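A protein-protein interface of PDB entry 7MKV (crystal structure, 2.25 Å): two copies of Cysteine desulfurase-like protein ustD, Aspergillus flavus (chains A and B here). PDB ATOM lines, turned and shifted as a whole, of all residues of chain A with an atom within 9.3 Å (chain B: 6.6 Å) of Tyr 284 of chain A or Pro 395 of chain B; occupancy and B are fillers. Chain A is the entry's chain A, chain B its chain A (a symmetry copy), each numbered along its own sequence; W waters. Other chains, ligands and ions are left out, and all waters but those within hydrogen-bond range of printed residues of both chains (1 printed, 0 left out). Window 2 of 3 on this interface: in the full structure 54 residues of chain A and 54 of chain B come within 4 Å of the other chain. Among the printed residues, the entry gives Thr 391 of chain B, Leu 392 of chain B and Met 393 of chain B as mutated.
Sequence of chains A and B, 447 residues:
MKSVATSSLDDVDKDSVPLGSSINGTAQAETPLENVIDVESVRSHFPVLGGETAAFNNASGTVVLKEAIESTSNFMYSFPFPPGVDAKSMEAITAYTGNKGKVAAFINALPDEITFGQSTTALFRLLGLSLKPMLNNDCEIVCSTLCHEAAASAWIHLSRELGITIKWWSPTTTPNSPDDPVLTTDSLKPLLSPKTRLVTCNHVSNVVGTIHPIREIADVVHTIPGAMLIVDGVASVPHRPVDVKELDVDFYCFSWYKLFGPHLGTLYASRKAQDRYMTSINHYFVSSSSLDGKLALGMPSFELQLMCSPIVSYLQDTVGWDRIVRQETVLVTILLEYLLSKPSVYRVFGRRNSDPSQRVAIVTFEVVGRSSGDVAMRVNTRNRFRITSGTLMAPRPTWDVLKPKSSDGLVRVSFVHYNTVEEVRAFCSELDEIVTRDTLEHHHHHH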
ATOM      1  N   SER A 280     -18.506 -18.958 -41.143  1.00  0.00           N
ATOM      2  CA  SER A 280     -19.505 -18.411 -40.188  1.00  0.00           C
ATOM      3  C   SER A 280     -19.552 -16.885 -40.300  1.00  0.00           C
ATOM      4  O   SER A 280     -18.469 -16.277 -40.353  1.00  0.00           O
ATOM      5  CB  SER A 280     -19.185 -18.830 -38.780  1.00  0.00           C
ATOM      6  OG  SER A 280     -20.042 -18.182 -37.861  1.00  0.00           O
ATOM      7  N   ILE A 281     -20.759 -16.307 -40.330  1.00  0.00           N
ATOM      8  CA  ILE A 281     -20.997 -14.831 -40.266  1.00  0.00           C
ATOM      9  C   ILE A 281     -21.562 -14.470 -38.885  1.00  0.00           C
ATOM     10  O   ILE A 281     -21.983 -13.316 -38.712  1.00  0.00           O
ATOM     11  CB  ILE A 281     -21.921 -14.365 -41.409  1.00  0.00           C
ATOM     12  CG1 ILE A 281     -23.354 -14.880 -41.259  1.00  0.00           C
ATOM     13  CG2 ILE A 281     -21.327 -14.742 -42.757  1.00  0.00           C
ATOM     14  CD1 ILE A 281     -24.346 -14.202 -42.178  1.00  0.00           C
ATOM     15  N   ASN A 282     -21.565 -15.427 -37.949  1.00  0.00           N
ATOM     16  CA  ASN A 282     -22.178 -15.312 -36.599  1.00  0.00           C
ATOM     17  C   ASN A 282     -21.093 -14.899 -35.595  1.00  0.00           C
ATOM     18  O   ASN A 282     -19.918 -14.811 -36.006  1.00  0.00           O
ATOM     19  CB  ASN A 282     -22.851 -16.630 -36.201  1.00  0.00           C
ATOM     20  CG  ASN A 282     -23.977 -16.474 -35.202  1.00  0.00           C
ATOM     21  OD1 ASN A 282     -24.120 -15.434 -34.565  1.00  0.00           O
ATOM     22  ND2 ASN A 282     -24.779 -17.516 -35.048  1.00  0.00           N
ATOM     23  N   HIS A 283     -21.479 -14.668 -34.334  1.00  0.00           N
ATOM     24  CA  HIS A 283     -20.574 -14.296 -33.212  1.00  0.00           C
ATOM     25  C   HIS A 283     -19.463 -15.344 -33.076  1.00  0.00           C
ATOM     26  O   HIS A 283     -19.741 -16.537 -33.314  1.00  0.00           O
ATOM     27  CB  HIS A 283     -21.353 -14.138 -31.896  1.00  0.00           C
ATOM     28  CG  HIS A 283     -22.609 -13.340 -32.015  1.00  0.00           C
ATOM     29  ND1 HIS A 283     -22.655 -12.127 -32.667  1.00  0.00           N
ATOM     30  CD2 HIS A 283     -23.861 -13.579 -31.572  1.00  0.00           C
ATOM     31  CE1 HIS A 283     -23.883 -11.652 -32.622  1.00  0.00           C
ATOM     32  NE2 HIS A 283     -24.644 -12.522 -31.952  1.00  0.00           N
ATOM     33  N   TYR A 284     -18.266 -14.913 -32.669  1.00  0.00           N
ATOM     34  CA  TYR A 284     -17.040 -15.753 -32.586  1.00  0.00           C
ATOM     35  C   TYR A 284     -17.272 -16.956 -31.661  1.00  0.00           C
ATOM     36  O   TYR A 284     -16.656 -18.001 -31.927  1.00  0.00           O
ATOM     37  CB  TYR A 284     -15.834 -14.920 -32.133  1.00  0.00           C
ATOM     38  CG  TYR A 284     -15.835 -14.519 -30.679  1.00  0.00           C
ATOM     39  CD1 TYR A 284     -15.358 -15.377 -29.699  1.00  0.00           C
ATOM     40  CD2 TYR A 284     -16.297 -13.277 -30.282  1.00  0.00           C
ATOM     41  CE1 TYR A 284     -15.352 -15.016 -28.362  1.00  0.00           C
ATOM     42  CE2 TYR A 284     -16.298 -12.899 -28.951  1.00  0.00           C
ATOM     43  CZ  TYR A 284     -15.823 -13.771 -27.986  1.00  0.00           C
ATOM     44  OH  TYR A 284     -15.814 -13.407 -26.671  1.00  0.00           O
ATOM     45  N   PHE A 285     -18.125 -16.812 -30.633  1.00  0.00           N
ATOM     46  CA  PHE A 285     -18.355 -17.816 -29.554  1.00  0.00           C
ATOM     47  C   PHE A 285     -19.392 -18.873 -29.972  1.00  0.00           C
ATOM     48  O   PHE A 285     -19.534 -19.867 -29.229  1.00  0.00           O
ATOM     49  CB  PHE A 285     -18.770 -17.139 -28.240  1.00  0.00           C
ATOM     50  CG  PHE A 285     -19.923 -16.166 -28.327  1.00  0.00           C
ATOM     51  CD1 PHE A 285     -21.235 -16.612 -28.418  1.00  0.00           C
ATOM     52  CD2 PHE A 285     -19.696 -14.798 -28.296  1.00  0.00           C
ATOM     53  CE1 PHE A 285     -22.288 -15.713 -28.495  1.00  0.00           C
ATOM     54  CE2 PHE A 285     -20.749 -13.900 -28.373  1.00  0.00           C
ATOM     55  CZ  PHE A 285     -22.043 -14.358 -28.473  1.00  0.00           C
ATOM     56  N   VAL A 286     -20.095 -18.682 -31.096  1.00  0.00           N
ATOM     57  CA  VAL A 286     -21.160 -19.617 -31.578  1.00  0.00           C
ATOM     58  C   VAL A 286     -20.509 -20.702 -32.447  1.00  0.00           C
ATOM     59  O   VAL A 286     -19.806 -20.345 -33.408  1.00  0.00           O
ATOM     60  CB  VAL A 286     -22.272 -18.872 -32.345  1.00  0.00           C
ATOM     61  CG1 VAL A 286     -23.317 -19.830 -32.902  1.00  0.00           C
ATOM     62  CG2 VAL A 286     -22.935 -17.807 -31.483  1.00  0.00           C
ATOM     63  N   SER A 287     -20.745 -21.976 -32.114  1.00  0.00           N
ATOM     64  CA  SER A 287     -20.261 -23.161 -32.872  1.00  0.00           C
ATOM     65  C   SER A 287     -20.771 -23.083 -34.318  1.00  0.00           C
ATOM     66  O   SER A 287     -21.967 -22.775 -34.510  1.00  0.00           O
ATOM     67  CB  SER A 287     -20.681 -24.447 -32.202  1.00  0.00           C
ATOM     68  OG  SER A 287     -20.297 -25.572 -32.980  1.00  0.00           O
ATOM     69  N   SER A 288     -19.894 -23.352 -35.291  1.00  0.00           N
ATOM     70  CA  SER A 288     -20.132 -23.125 -36.743  1.00  0.00           C
ATOM     71  C   SER A 288     -20.373 -24.452 -37.483  1.00  0.00           C
ATOM     72  O   SER A 288     -20.335 -24.433 -38.727  1.00  0.00           O
ATOM     73  CB  SER A 288     -18.980 -22.357 -37.345  1.00  0.00           C
ATOM     74  OG  SER A 288     -17.792 -23.134 -37.342  1.00  0.00           O
ATOM     75  N   GLY A 293     -25.670 -22.283 -36.894  1.00  0.00           N
ATOM     76  CA  GLY A 293     -24.429 -21.735 -36.312  1.00  0.00           C
ATOM     77  C   GLY A 293     -23.743 -20.747 -37.240  1.00  0.00           C
ATOM     78  O   GLY A 293     -23.237 -19.722 -36.740  1.00  0.00           O
ATOM     79  N   THR B 145     -17.308  -0.904 -25.465  1.00  0.00           N
ATOM     80  CA  THR B 145     -17.002  -2.275 -24.975  1.00  0.00           C
ATOM     81  C   THR B 145     -18.168  -2.796 -24.122  1.00  0.00           C
ATOM     82  O   THR B 145     -18.065  -3.941 -23.655  1.00  0.00           O
ATOM     83  CB  THR B 145     -15.664  -2.316 -24.226  1.00  0.00           C
ATOM     84  OG1 THR B 145     -15.734  -1.435 -23.108  1.00  0.00           O
ATOM     85  CG2 THR B 145     -14.491  -1.924 -25.096  1.00  0.00           C
ATOM     86  N   CSD B 147     -21.087  -3.020 -25.605  1.00  0.00           N
ATOM     87  CA  CSD B 147     -21.958  -3.430 -26.738  1.00  0.00           C
ATOM     88  CB  CSD B 147     -21.343  -3.075 -28.090  1.00  0.00           C
ATOM     89  SG  CSD B 147     -21.851  -1.397 -28.513  1.00  0.00           S
ATOM     90  C   CSD B 147     -22.250  -4.932 -26.684  1.00  0.00           C
ATOM     91  O   CSD B 147     -21.311  -5.719 -26.441  1.00  0.00           O
ATOM     92  OD1 CSD B 147     -21.275  -1.141 -29.857  1.00  0.00           O
ATOM     93  OD2 CSD B 147     -23.436  -1.420 -28.667  1.00  0.00           O
ATOM     94  N   HIS B 148     -23.514  -5.291 -26.913  1.00  0.00           N
ATOM     95  CA  HIS B 148     -23.985  -6.663 -27.241  1.00  0.00           C
ATOM     96  C   HIS B 148     -23.260  -7.118 -28.514  1.00  0.00           C
ATOM     97  O   HIS B 148     -22.961  -6.252 -29.351  1.00  0.00           O
ATOM     98  CB  HIS B 148     -25.514  -6.646 -27.398  1.00  0.00           C
ATOM     99  CG  HIS B 148     -26.165  -7.989 -27.387  1.00  0.00           C
ATOM    100  ND1 HIS B 148     -26.312  -8.752 -28.528  1.00  0.00           N
ATOM    101  CD2 HIS B 148     -26.751  -8.686 -26.390  1.00  0.00           C
ATOM    102  CE1 HIS B 148     -26.937  -9.872 -28.228  1.00  0.00           C
ATOM    103  NE2 HIS B 148     -27.220  -9.854 -26.924  1.00  0.00           N
ATOM    104  N   GLU B 149     -22.984  -8.417 -28.659  1.00  0.00           N
ATOM    105  CA  GLU B 149     -22.200  -8.955 -29.805  1.00  0.00           C
ATOM    106  C   GLU B 149     -23.005  -8.789 -31.101  1.00  0.00           C
ATOM    107  O   GLU B 149     -22.379  -8.733 -32.167  1.00  0.00           O
ATOM    108  CB  GLU B 149     -21.782 -10.408 -29.562  1.00  0.00           C
ATOM    109  CG  GLU B 149     -20.535 -10.816 -30.332  1.00  0.00           C
ATOM    110  CD  GLU B 149     -19.233 -10.156 -29.897  1.00  0.00           C
ATOM    111  OE1 GLU B 149     -19.262  -9.341 -28.957  1.00  0.00           O
ATOM    112  OE2 GLU B 149     -18.187 -10.461 -30.509  1.00  0.00           O
ATOM    113  N   SER B 153     -20.331  -7.700 -33.569  1.00  0.00           N
ATOM    114  CA  SER B 153     -20.154  -8.566 -34.767  1.00  0.00           C
ATOM    115  C   SER B 153     -20.377  -7.749 -36.043  1.00  0.00           C
ATOM    116  O   SER B 153     -19.614  -7.946 -36.996  1.00  0.00           O
ATOM    117  CB  SER B 153     -21.052  -9.776 -34.731  1.00  0.00           C
ATOM    118  OG  SER B 153     -20.570 -10.722 -33.790  1.00  0.00           O
ATOM    119  N   ILE B 156     -17.352  -5.209 -36.287  1.00  0.00           N
ATOM    120  CA  ILE B 156     -16.118  -6.025 -36.502  1.00  0.00           C
ATOM    121  C   ILE B 156     -16.087  -6.482 -37.965  1.00  0.00           C
ATOM    122  O   ILE B 156     -15.035  -6.326 -38.606  1.00  0.00           O
ATOM    123  CB  ILE B 156     -16.022  -7.208 -35.516  1.00  0.00           C
ATOM    124  CG1 ILE B 156     -15.668  -6.728 -34.108  1.00  0.00           C
ATOM    125  CG2 ILE B 156     -15.023  -8.249 -36.010  1.00  0.00           C
ATOM    126  CD1 ILE B 156     -15.894  -7.756 -33.024  1.00  0.00           C
ATOM    127  N   THR B 391     -22.802 -15.416 -19.983  1.00  0.00           N
ATOM    128  CA  THR B 391     -22.222 -14.262 -20.718  1.00  0.00           C
ATOM    129  C   THR B 391     -23.338 -13.482 -21.427  1.00  0.00           C
ATOM    130  O   THR B 391     -23.131 -12.292 -21.716  1.00  0.00           O
ATOM    131  CB  THR B 391     -21.139 -14.767 -21.677  1.00  0.00           C
ATOM    132  OG1 THR B 391     -20.218 -15.536 -20.904  1.00  0.00           O
ATOM    133  CG2 THR B 391     -20.396 -13.659 -22.386  1.00  0.00           C
ATOM    134  N   LEU B 392     -24.463 -14.142 -21.720  1.00  0.00           N
ATOM    135  CA  LEU B 392     -25.701 -13.537 -22.282  1.00  0.00           C
ATOM    136  C   LEU B 392     -25.388 -12.783 -23.581  1.00  0.00           C
ATOM    137  O   LEU B 392     -25.870 -11.640 -23.736  1.00  0.00           O
ATOM    138  CB  LEU B 392     -26.325 -12.622 -21.224  1.00  0.00           C
ATOM    139  CG  LEU B 392     -26.683 -13.308 -19.907  1.00  0.00           C
ATOM    140  CD1 LEU B 392     -27.036 -12.288 -18.840  1.00  0.00           C
ATOM    141  CD2 LEU B 392     -27.820 -14.297 -20.103  1.00  0.00           C
ATOM    142  N   MET B 393     -24.618 -13.414 -24.476  1.00  0.00           N
ATOM    143  CA  MET B 393     -24.332 -12.941 -25.860  1.00  0.00           C
ATOM    144  C   MET B 393     -23.614 -11.582 -25.806  1.00  0.00           C
ATOM    145  O   MET B 393     -23.723 -10.806 -26.778  1.00  0.00           O
ATOM    146  CB  MET B 393     -25.630 -12.808 -26.666  1.00  0.00           C
ATOM    147  CG  MET B 393     -26.521 -14.046 -26.633  1.00  0.00           C
ATOM    148  SD  MET B 393     -25.968 -15.366 -27.750  1.00  0.00           S
ATOM    149  CE  MET B 393     -26.280 -14.623 -29.349  1.00  0.00           C
ATOM    150  N   ALA B 394     -22.890 -11.319 -24.714  1.00  0.00           N
ATOM    151  CA  ALA B 394     -22.223 -10.030 -24.423  1.00  0.00           C
ATOM    152  C   ALA B 394     -20.905 -10.290 -23.700  1.00  0.00           C
ATOM    153  O   ALA B 394     -20.715  -9.848 -22.566  1.00  0.00           O
ATOM    154  CB  ALA B 394     -23.149  -9.155 -23.617  1.00  0.00           C
ATOM    155  N   PRO B 395     -19.948 -11.002 -24.339  1.00  0.00           N
ATOM    156  CA  PRO B 395     -18.657 -11.304 -23.714  1.00  0.00           C
ATOM    157  C   PRO B 395     -17.830 -10.072 -23.309  1.00  0.00           C
ATOM    158  O   PRO B 395     -17.111 -10.161 -22.331  1.00  0.00           O
ATOM    159  CB  PRO B 395     -17.909 -12.112 -24.787  1.00  0.00           C
ATOM    160  CG  PRO B 395     -18.604 -11.756 -26.085  1.00  0.00           C
ATOM    161  CD  PRO B 395     -20.053 -11.548 -25.700  1.00  0.00           C
ATOM    162  N   ARG B 396     -17.941  -8.968 -24.054  1.00  0.00           N
ATOM    163  CA  ARG B 396     -17.073  -7.772 -23.878  1.00  0.00           C
ATOM    164  C   ARG B 396     -17.473  -7.053 -22.590  1.00  0.00           C
ATOM    165  O   ARG B 396     -16.627  -6.836 -21.724  1.00  0.00           O
ATOM    166  CB  ARG B 396     -17.098  -6.901 -25.140  1.00  0.00           C
ATOM    167  CG  ARG B 396     -16.621  -7.635 -26.384  1.00  0.00           C
ATOM    168  CD  ARG B 396     -16.872  -6.916 -27.698  1.00  0.00           C
ATOM    169  NE  ARG B 396     -16.782  -7.872 -28.796  1.00  0.00           N
ATOM    170  CZ  ARG B 396     -15.651  -8.378 -29.288  1.00  0.00           C
ATOM    171  NH1 ARG B 396     -14.475  -8.008 -28.811  1.00  0.00           N
ATOM    172  NH2 ARG B 396     -15.703  -9.260 -30.269  1.00  0.00           N
ATOM    173  N   PRO B 397     -18.760  -6.690 -22.384  1.00  0.00           N
ATOM    174  CA  PRO B 397     -19.182  -6.088 -21.120  1.00  0.00           C
ATOM    175  C   PRO B 397     -18.997  -7.032 -19.920  1.00  0.00           C
ATOM    176  O   PRO B 397     -18.581  -6.579 -18.877  1.00  0.00           O
ATOM    177  CB  PRO B 397     -20.677  -5.777 -21.296  1.00  0.00           C
ATOM    178  CG  PRO B 397     -20.967  -5.965 -22.778  1.00  0.00           C
ATOM    179  CD  PRO B 397     -19.870  -6.842 -23.334  1.00  0.00           C
ATOM    180  N   THR B 398     -19.308  -8.319 -20.089  1.00  0.00           N
ATOM    181  CA  THR B 398     -19.252  -9.340 -19.011  1.00  0.00           C
ATOM    182  C   THR B 398     -17.795  -9.567 -18.586  1.00  0.00           C
ATOM    183  O   THR B 398     -17.500  -9.374 -17.393  1.00  0.00           O
ATOM    184  CB  THR B 398     -19.945 -10.641 -19.437  1.00  0.00           C
ATOM    185  OG1 THR B 398     -21.326 -10.352 -19.678  1.00  0.00           O
ATOM    186  CG2 THR B 398     -19.830 -11.740 -18.402  1.00  0.00           C
ATOM    187  N   TRP B 399     -16.913  -9.940 -19.517  1.00  0.00           N
ATOM    188  CA  TRP B 399     -15.557 -10.463 -19.192  1.00  0.00           C
ATOM    189  C   TRP B 399     -14.482  -9.367 -19.229  1.00  0.00           C
ATOM    190  O   TRP B 399     -13.440  -9.574 -18.576  1.00  0.00           O
ATOM    191  CB  TRP B 399     -15.204 -11.639 -20.109  1.00  0.00           C
ATOM    192  CG  TRP B 399     -16.038 -12.855 -19.844  1.00  0.00           C
ATOM    193  CD1 TRP B 399     -16.929 -13.445 -20.693  1.00  0.00           C
ATOM    194  CD2 TRP B 399     -16.079 -13.621 -18.626  1.00  0.00           C
ATOM    195  NE1 TRP B 399     -17.512 -14.528 -20.092  1.00  0.00           N
ATOM    196  CE2 TRP B 399     -17.011 -14.662 -18.824  1.00  0.00           C
ATOM    197  CE3 TRP B 399     -15.416 -13.536 -17.394  1.00  0.00           C
ATOM    198  CZ2 TRP B 399     -17.292 -15.606 -17.839  1.00  0.00           C
ATOM    199  CZ3 TRP B 399     -15.699 -14.468 -16.418  1.00  0.00           C
ATOM    200  CH2 TRP B 399     -16.624 -15.490 -16.642  1.00  0.00           C
ATOM    201  N   ASP B 400     -14.694  -8.262 -19.951  1.00  0.00           N
ATOM    202  CA  ASP B 400     -13.663  -7.198 -20.119  1.00  0.00           C
ATOM    203  C   ASP B 400     -13.966  -5.983 -19.226  1.00  0.00           C
ATOM    204  O   ASP B 400     -13.029  -5.203 -18.998  1.00  0.00           O
ATOM    205  CB  ASP B 400     -13.522  -6.772 -21.583  1.00  0.00           C
ATOM    206  CG  ASP B 400     -13.256  -7.917 -22.548  1.00  0.00           C
ATOM    207  OD1 ASP B 400     -12.603  -8.898 -22.137  1.00  0.00           O
ATOM    208  OD2 ASP B 400     -13.703  -7.813 -23.709  1.00  0.00           O
ATOM    209  N   VAL B 401     -15.205  -5.822 -18.744  1.00  0.00           N
ATOM    210  CA  VAL B 401     -15.630  -4.660 -17.901  1.00  0.00           C
ATOM    211  C   VAL B 401     -16.025  -5.154 -16.500  1.00  0.00           C
ATOM    212  O   VAL B 401     -15.315  -4.810 -15.539  1.00  0.00           O
ATOM    213  CB  VAL B 401     -16.770  -3.864 -18.566  1.00  0.00           C
ATOM    214  CG1 VAL B 401     -17.167  -2.653 -17.731  1.00  0.00           C
ATOM    215  CG2 VAL B 401     -16.411  -3.437 -19.981  1.00  0.00           C
HETATM  216  O   HOH W   1     -18.331 -11.776 -32.722  1.00  0.00           O
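ND1 of His 283 of chain A is in hydrogen-bond range of OG of Ser 153 of chain B (2.8 Å). The backbone carbonyl oxygen (O) of Glu 149 of chain B sits close to a ring nitrogen (ND1) of His 283 of chain A (3.4 Å).
OE2 of Glu 149 of chain B is in salt-bridge range of NH2 of Arg 396 of chain B (2.8 Å). N of Val 401 of chain B lies within hydrogen-bond range of O of Arg 396 of chain B (3.5 Å). The backbone NH (N) of Glu 149 of chain B lies within hydrogen-bond range of the backbone carbonyl oxygen (O) of Met 393 of chain B (3.1 Å). The backbone carbonyl oxygen (O) of Glu 149 of chain B lies close to the side-chain hydroxyl (OG) of Ser 153 of chain B (3.1 Å).
Among the printed residues, merely in contact across the chains: His 283 of chain A with Met 393 of chain B, Tyr 284 of chain A with Glu 149 of chain B, Tyr 284 of chain A with Pro 395 of chain B, Tyr 284 of chain A with Arg 396 of chain B, Phe 285 of chain A with Glu 149 of chain B, Phe 285 of chain A with Met 393 of chain B and Phe 285 of chain A with Pro 395 of chain B.
Of chain B, only Glu 149, Pro 395 and Arg 396 come within 4 Å of Tyr 284 of chain A. No residue of chain A comes within 4 Å of Ala 394 of chain B. No residue of chain A comes within 4 Å of Thr 398 of chain B. Printed residues of chain A within 4 Å of Glu 149 of chain B: His 283, Tyr 284 and Phe 285. Printed residues of chain A within 4 Å of Met 393 of chain B: His 283 and Phe 285. Printed residues of chain B within 4 Å of His 283 of chain A: Glu 149, Ser 153 and Met 393. Of the printed residues of chain A, Arg 396 of chain B touches Tyr 284 (3.9 Å). Of the printed residues of chain A, Ser 153 of chain B touches His 283. Ser 287 of chain A touches none of the printed residues of chain B. The nearest residue of chain B that does not touch Tyr 284 of chain A is Ser 153 of chain B (4.9 Å). The nearest residue of chain A that does not touch Pro 395 of chain B is His 283 of chain A (6.8 Å).
Of the 17 printed residues of chain B, 5 touch a printed residue of chain A. Among the printed residues, no Asp or Glu carboxylate lies within 4 Å of a Lys or Arg side-chain nitrogen of the other chain.
No position is printed for both chains.
Water W1 lies within hydrogen-bond range of the side-chain carboxylate of Glu 149 of chain B, the side-chain hydroxyl of Ser 153 of chain B and the backbone NH of Tyr 284 of chain A.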
